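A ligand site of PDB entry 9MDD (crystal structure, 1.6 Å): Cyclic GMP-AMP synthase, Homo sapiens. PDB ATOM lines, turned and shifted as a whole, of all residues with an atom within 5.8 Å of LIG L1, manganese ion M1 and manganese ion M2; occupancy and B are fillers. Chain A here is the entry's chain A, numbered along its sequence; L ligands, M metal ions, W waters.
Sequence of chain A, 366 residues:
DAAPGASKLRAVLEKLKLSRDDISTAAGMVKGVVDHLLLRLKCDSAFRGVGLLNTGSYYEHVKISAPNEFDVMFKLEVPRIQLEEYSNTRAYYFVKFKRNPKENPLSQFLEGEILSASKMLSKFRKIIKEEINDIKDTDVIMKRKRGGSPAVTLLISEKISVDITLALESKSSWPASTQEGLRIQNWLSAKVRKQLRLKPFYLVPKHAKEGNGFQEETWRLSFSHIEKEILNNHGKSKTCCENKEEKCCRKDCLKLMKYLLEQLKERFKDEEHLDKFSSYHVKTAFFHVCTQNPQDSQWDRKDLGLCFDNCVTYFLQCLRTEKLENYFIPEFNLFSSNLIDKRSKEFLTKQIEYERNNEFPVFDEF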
ATOM      1  N   THR A  55     -12.350   8.821  28.254  1.00  0.00           N
ATOM      2  CA  THR A  55     -12.897   8.008  29.330  1.00  0.00           C
ATOM      3  C   THR A  55     -12.911   6.545  28.911  1.00  0.00           C
ATOM      4  O   THR A  55     -12.577   6.199  27.779  1.00  0.00           O
ATOM      5  CB  THR A  55     -14.287   8.543  29.699  1.00  0.00           C
ATOM      6  OG1 THR A  55     -14.593   8.224  31.051  1.00  0.00           O
ATOM      7  CG2 THR A  55     -15.355   7.997  28.760  1.00  0.00           C
ATOM      8  N   GLY A  56     -13.295   5.658  29.848  1.00  0.00           N
ATOM      9  CA  GLY A  56     -13.416   4.260  29.499  1.00  0.00           C
ATOM     10  C   GLY A  56     -12.095   3.501  29.545  1.00  0.00           C
ATOM     11  O   GLY A  56     -11.040   4.014  29.937  1.00  0.00           O
ATOM     12  N   SER A  57     -12.167   2.243  29.104  1.00  0.00           N
ATOM     13  CA  SER A  57     -11.125   1.286  29.497  1.00  0.00           C
ATOM     14  C   SER A  57      -9.752   1.610  28.919  1.00  0.00           C
ATOM     15  O   SER A  57      -8.738   1.325  29.552  1.00  0.00           O
ATOM     16  CB  SER A  57     -11.536  -0.131  29.102  1.00  0.00           C
ATOM     17  OG  SER A  57     -11.516  -0.320  27.690  1.00  0.00           O
ATOM     18  N   TYR A  58      -9.671   2.189  27.715  1.00  0.00           N
ATOM     19  CA  TYR A  58      -8.348   2.513  27.189  1.00  0.00           C
ATOM     20  C   TYR A  58      -7.612   3.469  28.112  1.00  0.00           C
ATOM     21  O   TYR A  58      -6.418   3.290  28.387  1.00  0.00           O
ATOM     22  CB  TYR A  58      -8.474   3.112  25.794  1.00  0.00           C
ATOM     23  CG  TYR A  58      -7.136   3.468  25.173  1.00  0.00           C
ATOM     24  CD1 TYR A  58      -6.426   2.537  24.450  1.00  0.00           C
ATOM     25  CD2 TYR A  58      -6.611   4.756  25.287  1.00  0.00           C
ATOM     26  CE1 TYR A  58      -5.188   2.865  23.855  1.00  0.00           C
ATOM     27  CE2 TYR A  58      -5.380   5.093  24.709  1.00  0.00           C
ATOM     28  CZ  TYR A  58      -4.689   4.133  23.993  1.00  0.00           C
ATOM     29  OH  TYR A  58      -3.479   4.469  23.408  1.00  0.00           O
ATOM     30  N   LYS A  63      -8.135  -1.779  29.001  1.00  0.00           N
ATOM     31  CA  LYS A  63      -8.506  -2.303  27.696  1.00  0.00           C
ATOM     32  C   LYS A  63      -7.678  -3.563  27.414  1.00  0.00           C
ATOM     33  O   LYS A  63      -6.457  -3.555  27.587  1.00  0.00           O
ATOM     34  CB  LYS A  63      -8.251  -1.250  26.614  1.00  0.00           C
ATOM     35  CG  LYS A  63      -8.580  -1.747  25.191  1.00  0.00           C
ATOM     36  CD  LYS A  63     -10.064  -1.591  24.884  1.00  0.00           C
ATOM     37  CE  LYS A  63     -10.471  -2.240  23.573  1.00  0.00           C
ATOM     38  NZ  LYS A  63     -10.393  -3.731  23.559  1.00  0.00           N
ATOM     39  N   GLU A  69     -11.102   0.030  20.627  1.00  0.00           N
ATOM     40  CA  GLU A  69     -12.366   0.637  21.074  1.00  0.00           C
ATOM     41  C   GLU A  69     -12.052   1.742  22.074  1.00  0.00           C
ATOM     42  O   GLU A  69     -11.466   1.513  23.142  1.00  0.00           O
ATOM     43  CB  GLU A  69     -13.293  -0.412  21.698  1.00  0.00           C
ATOM     44  CG  GLU A  69     -14.801  -0.007  21.618  1.00  0.00           C
ATOM     45  CD  GLU A  69     -15.314   0.738  22.844  1.00  0.00           C
ATOM     46  OE1 GLU A  69     -14.513   1.020  23.743  1.00  0.00           O
ATOM     47  OE2 GLU A  69     -16.545   1.024  22.879  1.00  0.00           O
ATOM     48  N   PHE A  70     -12.401   2.973  21.701  1.00  0.00           N
ATOM     49  CA  PHE A  70     -12.116   4.150  22.487  1.00  0.00           C
ATOM     50  C   PHE A  70     -13.418   4.872  22.824  1.00  0.00           C
ATOM     51  O   PHE A  70     -14.328   4.900  21.995  1.00  0.00           O
ATOM     52  CB  PHE A  70     -11.247   5.139  21.719  1.00  0.00           C
ATOM     53  CG  PHE A  70      -9.852   4.645  21.426  1.00  0.00           C
ATOM     54  CD1 PHE A  70      -9.643   3.707  20.418  1.00  0.00           C
ATOM     55  CD2 PHE A  70      -8.756   5.134  22.131  1.00  0.00           C
ATOM     56  CE1 PHE A  70      -8.377   3.268  20.120  1.00  0.00           C
ATOM     57  CE2 PHE A  70      -7.479   4.696  21.825  1.00  0.00           C
ATOM     58  CZ  PHE A  70      -7.299   3.751  20.811  1.00  0.00           C
ATOM     59  N   ASP A  71     -13.448   5.521  23.989  1.00  0.00           N
ATOM     60  CA  ASP A  71     -14.596   6.298  24.436  1.00  0.00           C
ATOM     61  C   ASP A  71     -14.173   7.731  24.733  1.00  0.00           C
ATOM     62  O   ASP A  71     -13.168   7.943  25.398  1.00  0.00           O
ATOM     63  CB  ASP A  71     -15.201   5.656  25.685  1.00  0.00           C
ATOM     64  CG  ASP A  71     -15.571   4.221  25.444  1.00  0.00           C
ATOM     65  OD1 ASP A  71     -16.548   3.969  24.704  1.00  0.00           O
ATOM     66  OD2 ASP A  71     -14.826   3.336  25.967  1.00  0.00           O
ATOM     67  N   VAL A  72     -14.939   8.698  24.231  1.00  0.00           N
ATOM     68  CA  VAL A  72     -14.630  10.095  24.494  1.00  0.00           C
ATOM     69  C   VAL A  72     -15.942  10.837  24.698  1.00  0.00           C
ATOM     70  O   VAL A  72     -16.902  10.615  23.971  1.00  0.00           O
ATOM     71  CB  VAL A  72     -13.805  10.728  23.352  1.00  0.00           C
ATOM     72  CG1 VAL A  72     -14.581  10.688  22.037  1.00  0.00           C
ATOM     73  CG2 VAL A  72     -13.456  12.165  23.703  1.00  0.00           C
ATOM     74  N   MET A  73     -15.958  11.706  25.704  1.00  0.00           N
ATOM     75  CA  MET A  73     -17.102  12.574  25.961  1.00  0.00           C
ATOM     76  C   MET A  73     -16.841  13.918  25.297  1.00  0.00           C
ATOM     77  O   MET A  73     -15.743  14.480  25.431  1.00  0.00           O
ATOM     78  CB  MET A  73     -17.263  12.738  27.467  1.00  0.00           C
ATOM     79  CG  MET A  73     -17.387  11.367  28.135  1.00  0.00           C
ATOM     80  SD  MET A  73     -17.486  11.493  29.920  1.00  0.00           S
ATOM     81  CE  MET A  73     -19.054  12.330  30.053  1.00  0.00           C
ATOM     82  N   ARG A 146     -26.935   2.230  17.672  1.00  0.00           N
ATOM     83  CA  ARG A 146     -26.871   1.109  18.597  1.00  0.00           C
ATOM     84  C   ARG A 146     -27.913   1.371  19.674  1.00  0.00           C
ATOM     85  O   ARG A 146     -27.784   2.327  20.449  1.00  0.00           O
ATOM     86  CB  ARG A 146     -25.456   0.995  19.178  1.00  0.00           C
ATOM     87  CG  ARG A 146     -25.169  -0.168  20.122  1.00  0.00           C
ATOM     88  CD  ARG A 146     -23.654  -0.288  20.386  1.00  0.00           C
ATOM     89  NE  ARG A 146     -23.129   0.878  21.074  1.00  0.00           N
ATOM     90  CZ  ARG A 146     -21.873   1.317  21.021  1.00  0.00           C
ATOM     91  NH1 ARG A 146     -20.964   0.732  20.256  1.00  0.00           N
ATOM     92  NH2 ARG A 146     -21.521   2.375  21.740  1.00  0.00           N
ATOM     93  N   GLY A 147     -28.959   0.544  19.723  1.00  0.00           N
ATOM     94  CA  GLY A 147     -30.043   0.759  20.667  1.00  0.00           C
ATOM     95  C   GLY A 147     -29.592   1.153  22.069  1.00  0.00           C
ATOM     96  O   GLY A 147     -28.669   0.553  22.624  1.00  0.00           O
ATOM     97  N   GLY A 148     -30.235   2.177  22.638  1.00  0.00           N
ATOM     98  CA  GLY A 148     -29.907   2.603  23.979  1.00  0.00           C
ATOM     99  C   GLY A 148     -28.509   3.165  24.161  1.00  0.00           C
ATOM    100  O   GLY A 148     -28.008   3.246  25.284  1.00  0.00           O
ATOM    101  N   SER A 149     -27.858   3.532  23.085  1.00  0.00           N
ATOM    102  CA  SER A 149     -26.536   4.111  23.267  1.00  0.00           C
ATOM    103  C   SER A 149     -26.634   5.624  23.251  1.00  0.00           C
ATOM    104  O   SER A 149     -27.297   6.171  22.355  1.00  0.00           O
ATOM    105  CB  SER A 149     -25.592   3.650  22.153  1.00  0.00           C
ATOM    106  OG  SER A 149     -24.404   4.412  22.142  1.00  0.00           O
ATOM    107  N   PRO A 150     -26.011   6.335  24.191  1.00  0.00           N
ATOM    108  CA  PRO A 150     -25.936   7.793  24.076  1.00  0.00           C
ATOM    109  C   PRO A 150     -24.843   8.266  23.128  1.00  0.00           C
ATOM    110  O   PRO A 150     -24.667   9.468  22.970  1.00  0.00           O
ATOM    111  CB  PRO A 150     -25.629   8.244  25.503  1.00  0.00           C
ATOM    112  CG  PRO A 150     -24.821   7.118  26.069  1.00  0.00           C
ATOM    113  CD  PRO A 150     -25.314   5.844  25.390  1.00  0.00           C
ATOM    114  N   ALA A 151     -24.103   7.346  22.515  1.00  0.00           N
ATOM    115  CA  ALA A 151     -22.929   7.697  21.731  1.00  0.00           C
ATOM    116  C   ALA A 151     -23.256   7.737  20.239  1.00  0.00           C
ATOM    117  O   ALA A 151     -24.234   7.153  19.769  1.00  0.00           O
ATOM    118  CB  ALA A 151     -21.786   6.700  21.981  1.00  0.00           C
ATOM    119  N   ASP A 163     -16.474   5.700  20.349  1.00  0.00           N
ATOM    120  CA  ASP A 163     -17.787   6.135  20.822  1.00  0.00           C
ATOM    121  C   ASP A 163     -17.673   7.565  21.318  1.00  0.00           C
ATOM    122  O   ASP A 163     -16.998   7.811  22.321  1.00  0.00           O
ATOM    123  CB  ASP A 163     -18.296   5.261  21.955  1.00  0.00           C
ATOM    124  CG  ASP A 163     -18.628   3.873  21.514  1.00  0.00           C
ATOM    125  OD1 ASP A 163     -19.079   3.675  20.376  1.00  0.00           O
ATOM    126  OD2 ASP A 163     -18.514   2.954  22.361  1.00  0.00           O
ATOM    127  N   THR A 165     -19.633  10.556  22.948  1.00  0.00           N
ATOM    128  CA  THR A 165     -20.845  10.785  23.733  1.00  0.00           C
ATOM    129  C   THR A 165     -20.979  12.264  24.066  1.00  0.00           C
ATOM    130  O   THR A 165     -20.134  12.824  24.774  1.00  0.00           O
ATOM    131  CB  THR A 165     -20.836   9.931  25.006  1.00  0.00           C
ATOM    132  OG1 THR A 165     -20.753   8.555  24.648  1.00  0.00           O
ATOM    133  CG2 THR A 165     -22.105  10.152  25.834  1.00  0.00           C
ATOM    134  N   VAL A 204     -25.919  12.422  29.920  1.00  0.00           N
ATOM    135  CA  VAL A 204     -25.750  11.931  28.555  1.00  0.00           C
ATOM    136  C   VAL A 204     -27.124  11.589  27.981  1.00  0.00           C
ATOM    137  O   VAL A 204     -28.071  11.349  28.740  1.00  0.00           O
ATOM    138  CB  VAL A 204     -24.797  10.719  28.506  1.00  0.00           C
ATOM    139  CG1 VAL A 204     -23.421  11.129  29.045  1.00  0.00           C
ATOM    140  CG2 VAL A 204     -25.373   9.510  29.271  1.00  0.00           C
ATOM    141  N   LYS A 206     -29.126   9.322  27.058  1.00  0.00           N
ATOM    142  CA  LYS A 206     -29.705   7.995  27.148  1.00  0.00           C
ATOM    143  C   LYS A 206     -31.046   8.135  27.850  1.00  0.00           C
ATOM    144  O   LYS A 206     -31.128   8.747  28.921  1.00  0.00           O
ATOM    145  CB  LYS A 206     -28.768   7.026  27.891  1.00  0.00           C
ATOM    146  CG  LYS A 206     -29.369   5.670  28.142  1.00  0.00           C
ATOM    147  CD  LYS A 206     -28.293   4.690  28.536  1.00  0.00           C
ATOM    148  CE  LYS A 206     -28.936   3.449  29.092  1.00  0.00           C
ATOM    149  NZ  LYS A 206     -28.837   2.405  28.041  1.00  0.00           N
ATOM    150  N   ARG A 220     -29.459  10.921  31.221  1.00  0.00           N
ATOM    151  CA  ARG A 220     -29.017   9.991  32.251  1.00  0.00           C
ATOM    152  C   ARG A 220     -27.705  10.447  32.862  1.00  0.00           C
ATOM    153  O   ARG A 220     -26.822  10.958  32.162  1.00  0.00           O
ATOM    154  CB  ARG A 220     -28.853   8.580  31.679  1.00  0.00           C
ATOM    155  CG  ARG A 220     -28.446   7.557  32.747  1.00  0.00           C
ATOM    156  CD  ARG A 220     -28.949   6.167  32.470  1.00  0.00           C
ATOM    157  NE  ARG A 220     -28.108   5.180  33.139  1.00  0.00           N
ATOM    158  CZ  ARG A 220     -28.286   3.863  33.095  1.00  0.00           C
ATOM    159  NH1 ARG A 220     -29.333   3.329  32.479  1.00  0.00           N
ATOM    160  NH2 ARG A 220     -27.384   3.062  33.653  1.00  0.00           N
ATOM    161  N   LEU A 221     -27.577  10.256  34.172  1.00  0.00           N
ATOM    162  CA  LEU A 221     -26.340  10.603  34.861  1.00  0.00           C
ATOM    163  C   LEU A 221     -25.206   9.705  34.379  1.00  0.00           C
ATOM    164  O   LEU A 221     -25.383   8.502  34.180  1.00  0.00           O
ATOM    165  CB  LEU A 221     -26.551  10.404  36.362  1.00  0.00           C
ATOM    166  CG  LEU A 221     -27.181  11.566  37.124  1.00  0.00           C
ATOM    167  CD1 LEU A 221     -27.317  11.222  38.610  1.00  0.00           C
ATOM    168  CD2 LEU A 221     -26.440  12.883  36.932  1.00  0.00           C
ATOM    169  N   SER A 222     -24.013  10.290  34.202  1.00  0.00           N
ATOM    170  CA  SER A 222     -22.818   9.495  33.961  1.00  0.00           C
ATOM    171  C   SER A 222     -21.707   9.964  34.872  1.00  0.00           C
ATOM    172  O   SER A 222     -21.468  11.169  34.997  1.00  0.00           O
ATOM    173  CB  SER A 222     -22.374   9.588  32.492  1.00  0.00           C
ATOM    174  OG  SER A 222     -21.161   8.838  32.304  1.00  0.00           O
ATOM    175  N   SER A 224     -18.592   8.363  34.406  1.00  0.00           N
ATOM    176  CA  SER A 224     -17.481   7.695  33.746  1.00  0.00           C
ATOM    177  C   SER A 224     -16.161   8.355  34.121  1.00  0.00           C
ATOM    178  O   SER A 224     -15.134   7.666  34.273  1.00  0.00           O
ATOM    179  CB  SER A 224     -17.684   7.719  32.224  1.00  0.00           C
ATOM    180  OG  SER A 224     -16.765   6.878  31.551  1.00  0.00           O
ATOM    181  N   SER A 278     -22.972  -6.410  29.862  1.00  0.00           N
ATOM    182  CA  SER A 278     -21.886  -5.654  29.272  1.00  0.00           C
ATOM    183  C   SER A 278     -20.737  -5.560  30.253  1.00  0.00           C
ATOM    184  O   SER A 278     -20.844  -5.950  31.429  1.00  0.00           O
ATOM    185  CB  SER A 278     -22.308  -4.232  28.866  1.00  0.00           C
ATOM    186  OG  SER A 278     -22.357  -3.386  29.992  1.00  0.00           O
HETATM  187  C1  LIG L   1     -24.870   2.209  27.400  1.00  0.00           C
HETATM  188  C2  LIG L   1     -22.480   5.015  28.213  1.00  0.00           C
HETATM  189  C3  LIG L   1     -23.205   6.424  30.032  1.00  0.00           C
HETATM  190  C4  LIG L   1     -24.498   4.466  29.356  1.00  0.00           C
HETATM  191  C5  LIG L   1     -19.313   7.914  27.997  1.00  0.00           C
HETATM  192  C6  LIG L   1     -19.623   8.484  29.211  1.00  0.00           C
HETATM  193  C7  LIG L   1     -22.743  -0.115  26.890  1.00  0.00           C
HETATM  194  C8  LIG L   1     -20.499   2.505  25.220  1.00  0.00           C
HETATM  195  C9  LIG L   1     -19.237  -0.570  23.549  1.00  0.00           C
HETATM  196  C10 LIG L   1     -20.515   1.113  24.549  1.00  0.00           C
HETATM  197  C11 LIG L   1     -21.713   0.336  24.375  1.00  0.00           C
HETATM  198  C12 LIG L   1     -21.575  -0.909  23.777  1.00  0.00           C
HETATM  199  C13 LIG L   1     -20.355  -1.390  23.354  1.00  0.00           C
HETATM  200  C14 LIG L   1     -23.034   0.843  24.770  1.00  0.00           C
HETATM  201  C15 LIG L   1     -24.889   1.005  26.440  1.00  0.00           C
HETATM  202  C16 LIG L   1     -23.589   4.165  28.346  1.00  0.00           C
HETATM  203  C17 LIG L   1     -22.312   6.131  29.025  1.00  0.00           C
HETATM  204  C18 LIG L   1     -24.267   5.572  30.148  1.00  0.00           C
HETATM  205  C19 LIG L   1     -21.164   6.997  28.873  1.00  0.00           C
HETATM  206  C20 LIG L   1     -25.662  -0.038  27.199  1.00  0.00           C
HETATM  207  N1  LIG L   1     -19.329   0.627  24.141  1.00  0.00           N
HETATM  208  N2  LIG L   1     -23.568   0.566  26.031  1.00  0.00           N
HETATM  209  N3  LIG L   1     -23.724   3.036  27.494  1.00  0.00           N
HETATM  210  N4  LIG L   1     -20.313   6.979  27.764  1.00  0.00           N
HETATM  211  N5  LIG L   1     -20.766   7.915  29.753  1.00  0.00           N
HETATM  212  O1  LIG L   1     -25.838   2.394  28.094  1.00  0.00           O
HETATM  213  O2  LIG L   1     -23.688   1.439  23.995  1.00  0.00           O
HETATM  214  O3  LIG L   1     -21.544   2.863  25.782  1.00  0.00           O
HETATM  215  O4  LIG L   1     -19.423   3.105  25.123  1.00  0.00           O
HETATM  216 CL1  LIG L   1     -25.420   5.930  31.419  1.00  0.00          CL
HETATM  217  P1  LG2 L   2     -14.499  -1.987  27.225  1.00  0.00           P
HETATM  218  O1  LG2 L   2     -14.623  -0.960  26.127  1.00  0.00           O
HETATM  219  O2  LG2 L   2     -13.026  -2.396  27.342  1.00  0.00           O
HETATM  220  O3  LG2 L   2     -15.387  -3.263  26.951  1.00  0.00           O
HETATM  221  P2  LG2 L   2     -15.420   0.242  28.932  1.00  0.00           P
HETATM  222  O4  LG2 L   2     -15.393   0.551  30.393  1.00  0.00           O
HETATM  223  O5  LG2 L   2     -14.608   1.227  28.062  1.00  0.00           O
HETATM  224  N1  LG2 L   2     -14.943  -1.357  28.726  1.00  0.00           N
HETATM  225  P3  LG2 L   2     -17.798   0.831  27.302  1.00  0.00           P
HETATM  226  O6  LG2 L   2     -18.904  -0.141  27.086  1.00  0.00           O
HETATM  227  O7  LG2 L   2     -16.963   1.179  26.041  1.00  0.00           O
HETATM  228  O8  LG2 L   2     -16.940   0.263  28.528  1.00  0.00           O
HETATM  229  O9  LG2 L   2     -18.449   2.127  27.914  1.00  0.00           O
HETATM  230  C1  LG2 L   2     -17.695   3.331  28.094  1.00  0.00           C
HETATM  231  C2  LG2 L   2     -18.035   3.912  29.457  1.00  0.00           C
HETATM  232  O10 LG2 L   2     -19.432   4.259  29.483  1.00  0.00           O
HETATM  233  C3  LG2 L   2     -17.864   2.975  30.655  1.00  0.00           C
HETATM  234  O11 LG2 L   2     -16.523   2.913  31.135  1.00  0.00           O
HETATM  235  C4  LG2 L   2     -18.800   3.611  31.679  1.00  0.00           C
HETATM  236  O12 LG2 L   2     -18.186   4.688  32.387  1.00  0.00           O
HETATM  237  C5  LG2 L   2     -19.946   4.109  30.802  1.00  0.00           C
HETATM  238  N2  LG2 L   2     -21.043   3.152  30.771  1.00  0.00           N
HETATM  239  C6  LG2 L   2     -21.190   2.065  29.951  1.00  0.00           C
HETATM  240  N3  LG2 L   2     -22.239   1.337  30.220  1.00  0.00           N
HETATM  241  C7  LG2 L   2     -22.836   1.987  31.288  1.00  0.00           C
HETATM  242  C8  LG2 L   2     -23.994   1.720  32.033  1.00  0.00           C
HETATM  243  N4  LG2 L   2     -24.804   0.676  31.819  1.00  0.00           N
HETATM  244  N5  LG2 L   2     -24.293   2.569  33.044  1.00  0.00           N
HETATM  245  C9  LG2 L   2     -23.479   3.599  33.290  1.00  0.00           C
HETATM  246  N6  LG2 L   2     -22.362   3.948  32.653  1.00  0.00           N
HETATM  247  C10 LG2 L   2     -22.095   3.095  31.657  1.00  0.00           C
HETATM  248 MN    MN M   1     -17.692   2.199  24.184  1.00  0.00          MN
HETATM  249 MN    MN M   2     -14.741   1.182  25.890  1.00  0.00          MN
HETATM  250  O   HOH W   1     -20.142   5.564  25.250  1.00  0.00           O
HETATM  251  O   HOH W   2     -18.168   7.609  24.856  1.00  0.00           O
HETATM  252  O   HOH W   3     -12.409   1.377  25.794  1.00  0.00           O
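The side-chain amino group (NZ) of Lys 206 is in hydrogen-bond range of an oxygen (O1) of LIG L1, 3.0 Å away. An oxygen (O2) of LIG L1 lies within hydrogen-bond range of the guanidinium group (NE) of Arg 146 (3.0 Å). The side-chain hydroxyl of Ser 222 lies within hydrogen-bond range of a nitrogen (N5) of LIG L1, at 2.7 Å. The side-chain hydroxyl of Ser 224 sits at hydrogen-bond distance from an oxygen (O12) of LG2 L2, at 2.7 Å. The backbone NH (N) of Ser 57 lies close to an oxygen (O5) of LG2 L2, at 2.8 Å. The guanidinium group (NH2) of Arg 220 lies within hydrogen-bond range of a nitrogen (N5) of LG2 L2 (3.2 Å). The side-chain hydroxyl of Ser 57 lies within hydrogen-bond range of an oxygen (O2) of LG2 L2.
OG of Ser 222 is in hydrogen-bond range of N of Ser 224. N of Thr 55 lies within hydrogen-bond range of O of Asp 71 (3.1 Å). OD1 of Asp 163 is in salt-bridge range of NH2 of Arg 146. N of Thr 165 sits at hydrogen-bond distance from O of Val 72, 2.9 Å away. The backbone carbonyl oxygen (O) of Arg 220 sits at hydrogen-bond distance from the backbone NH (N) of Val 204, at 2.8 Å. The backbone carbonyl oxygen (O) of Asp 163 is in hydrogen-bond range of the backbone NH (N) of Val 72 (2.9 Å). The side-chain hydroxyl (OG) of Ser 149 sits at hydrogen-bond distance from the backbone NH (N) of Ala 151 (3.0 Å). N of Asp 163 lies within hydrogen-bond range of O of Phe 70 (2.8 Å).
Residues that only touch LIG L1: Met 73 (3.8 Å), Gly 148 (3.7 Å), Ser 149 (3.5 Å), Pro 150 (3.8 Å), Thr 165 (3.5 Å), Val 204 (3.8 Å), Arg 220 (3.3 Å), Leu 221 (3.8 Å) and Ser 224 (3.7 Å). Hydrophobic or aromatic side chains within 4 Å of LIG L1: Met 73, Pro 150 and Val 204.
Within 4 Å of manganese ion M1: Glu 69, Asp 71 and Asp 163.
Merely in contact with manganese ion M2: Ser 57. Three residues have an atom within 4 Å of manganese ion M2: Ser 57, Glu 69 and Asp 71. Along chain A the residues within 4 Å of manganese ion M2 span positions 57 to 71. The nearest printed residue that does not touch manganese ion M2 is Gly 56 (4.9 Å).
OE2 of Glu 69 is bound to manganese ion M1. OD2 of Asp 163 binds manganese ion M1 (2.1 Å). O4 of LIG L1 is bound to manganese ion M1. OD1 of Asp 71 is bound to manganese ion M1 (2.2 Å). Manganese ion M1 is bound by an oxygen (O7) of LG2 L2. N1 of LIG L1 binds manganese ion M1. Manganese ion M1 has six donor atoms within binding distance.
OD2 of Asp 71 is bound to manganese ion M2, 2.2 Å away. O1 of LG2 L2 binds manganese ion M2 (2.2 Å). Manganese ion M2 is bound by the side-chain carboxylate (OE1) of Glu 69 (2.2 Å). O5 of LG2 L2 is bound to manganese ion M2. O7 of LG2 L2 binds manganese ion M2. Manganese ion M2 is bound by water W3. Manganese ion M2 has six donor atoms within binding distance.
Water W3 lies within hydrogen-bond range of OG of Ser 57 (2.7 Å), O of Glu 69 (2.8 Å) and N of Tyr 58 (3.4 Å). Water W1 lies within hydrogen-bond range of a nitrogen (N4) of LIG L1 (2.9 Å) and the side-chain hydroxyl (OG1) of Thr 165 (3.1 Å). Water W2 lies within hydrogen-bond range of OG1 of Thr 165 (2.8 Å), O of Asp 163 (2.8 Å) and O of Val 72 (3.4 Å).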
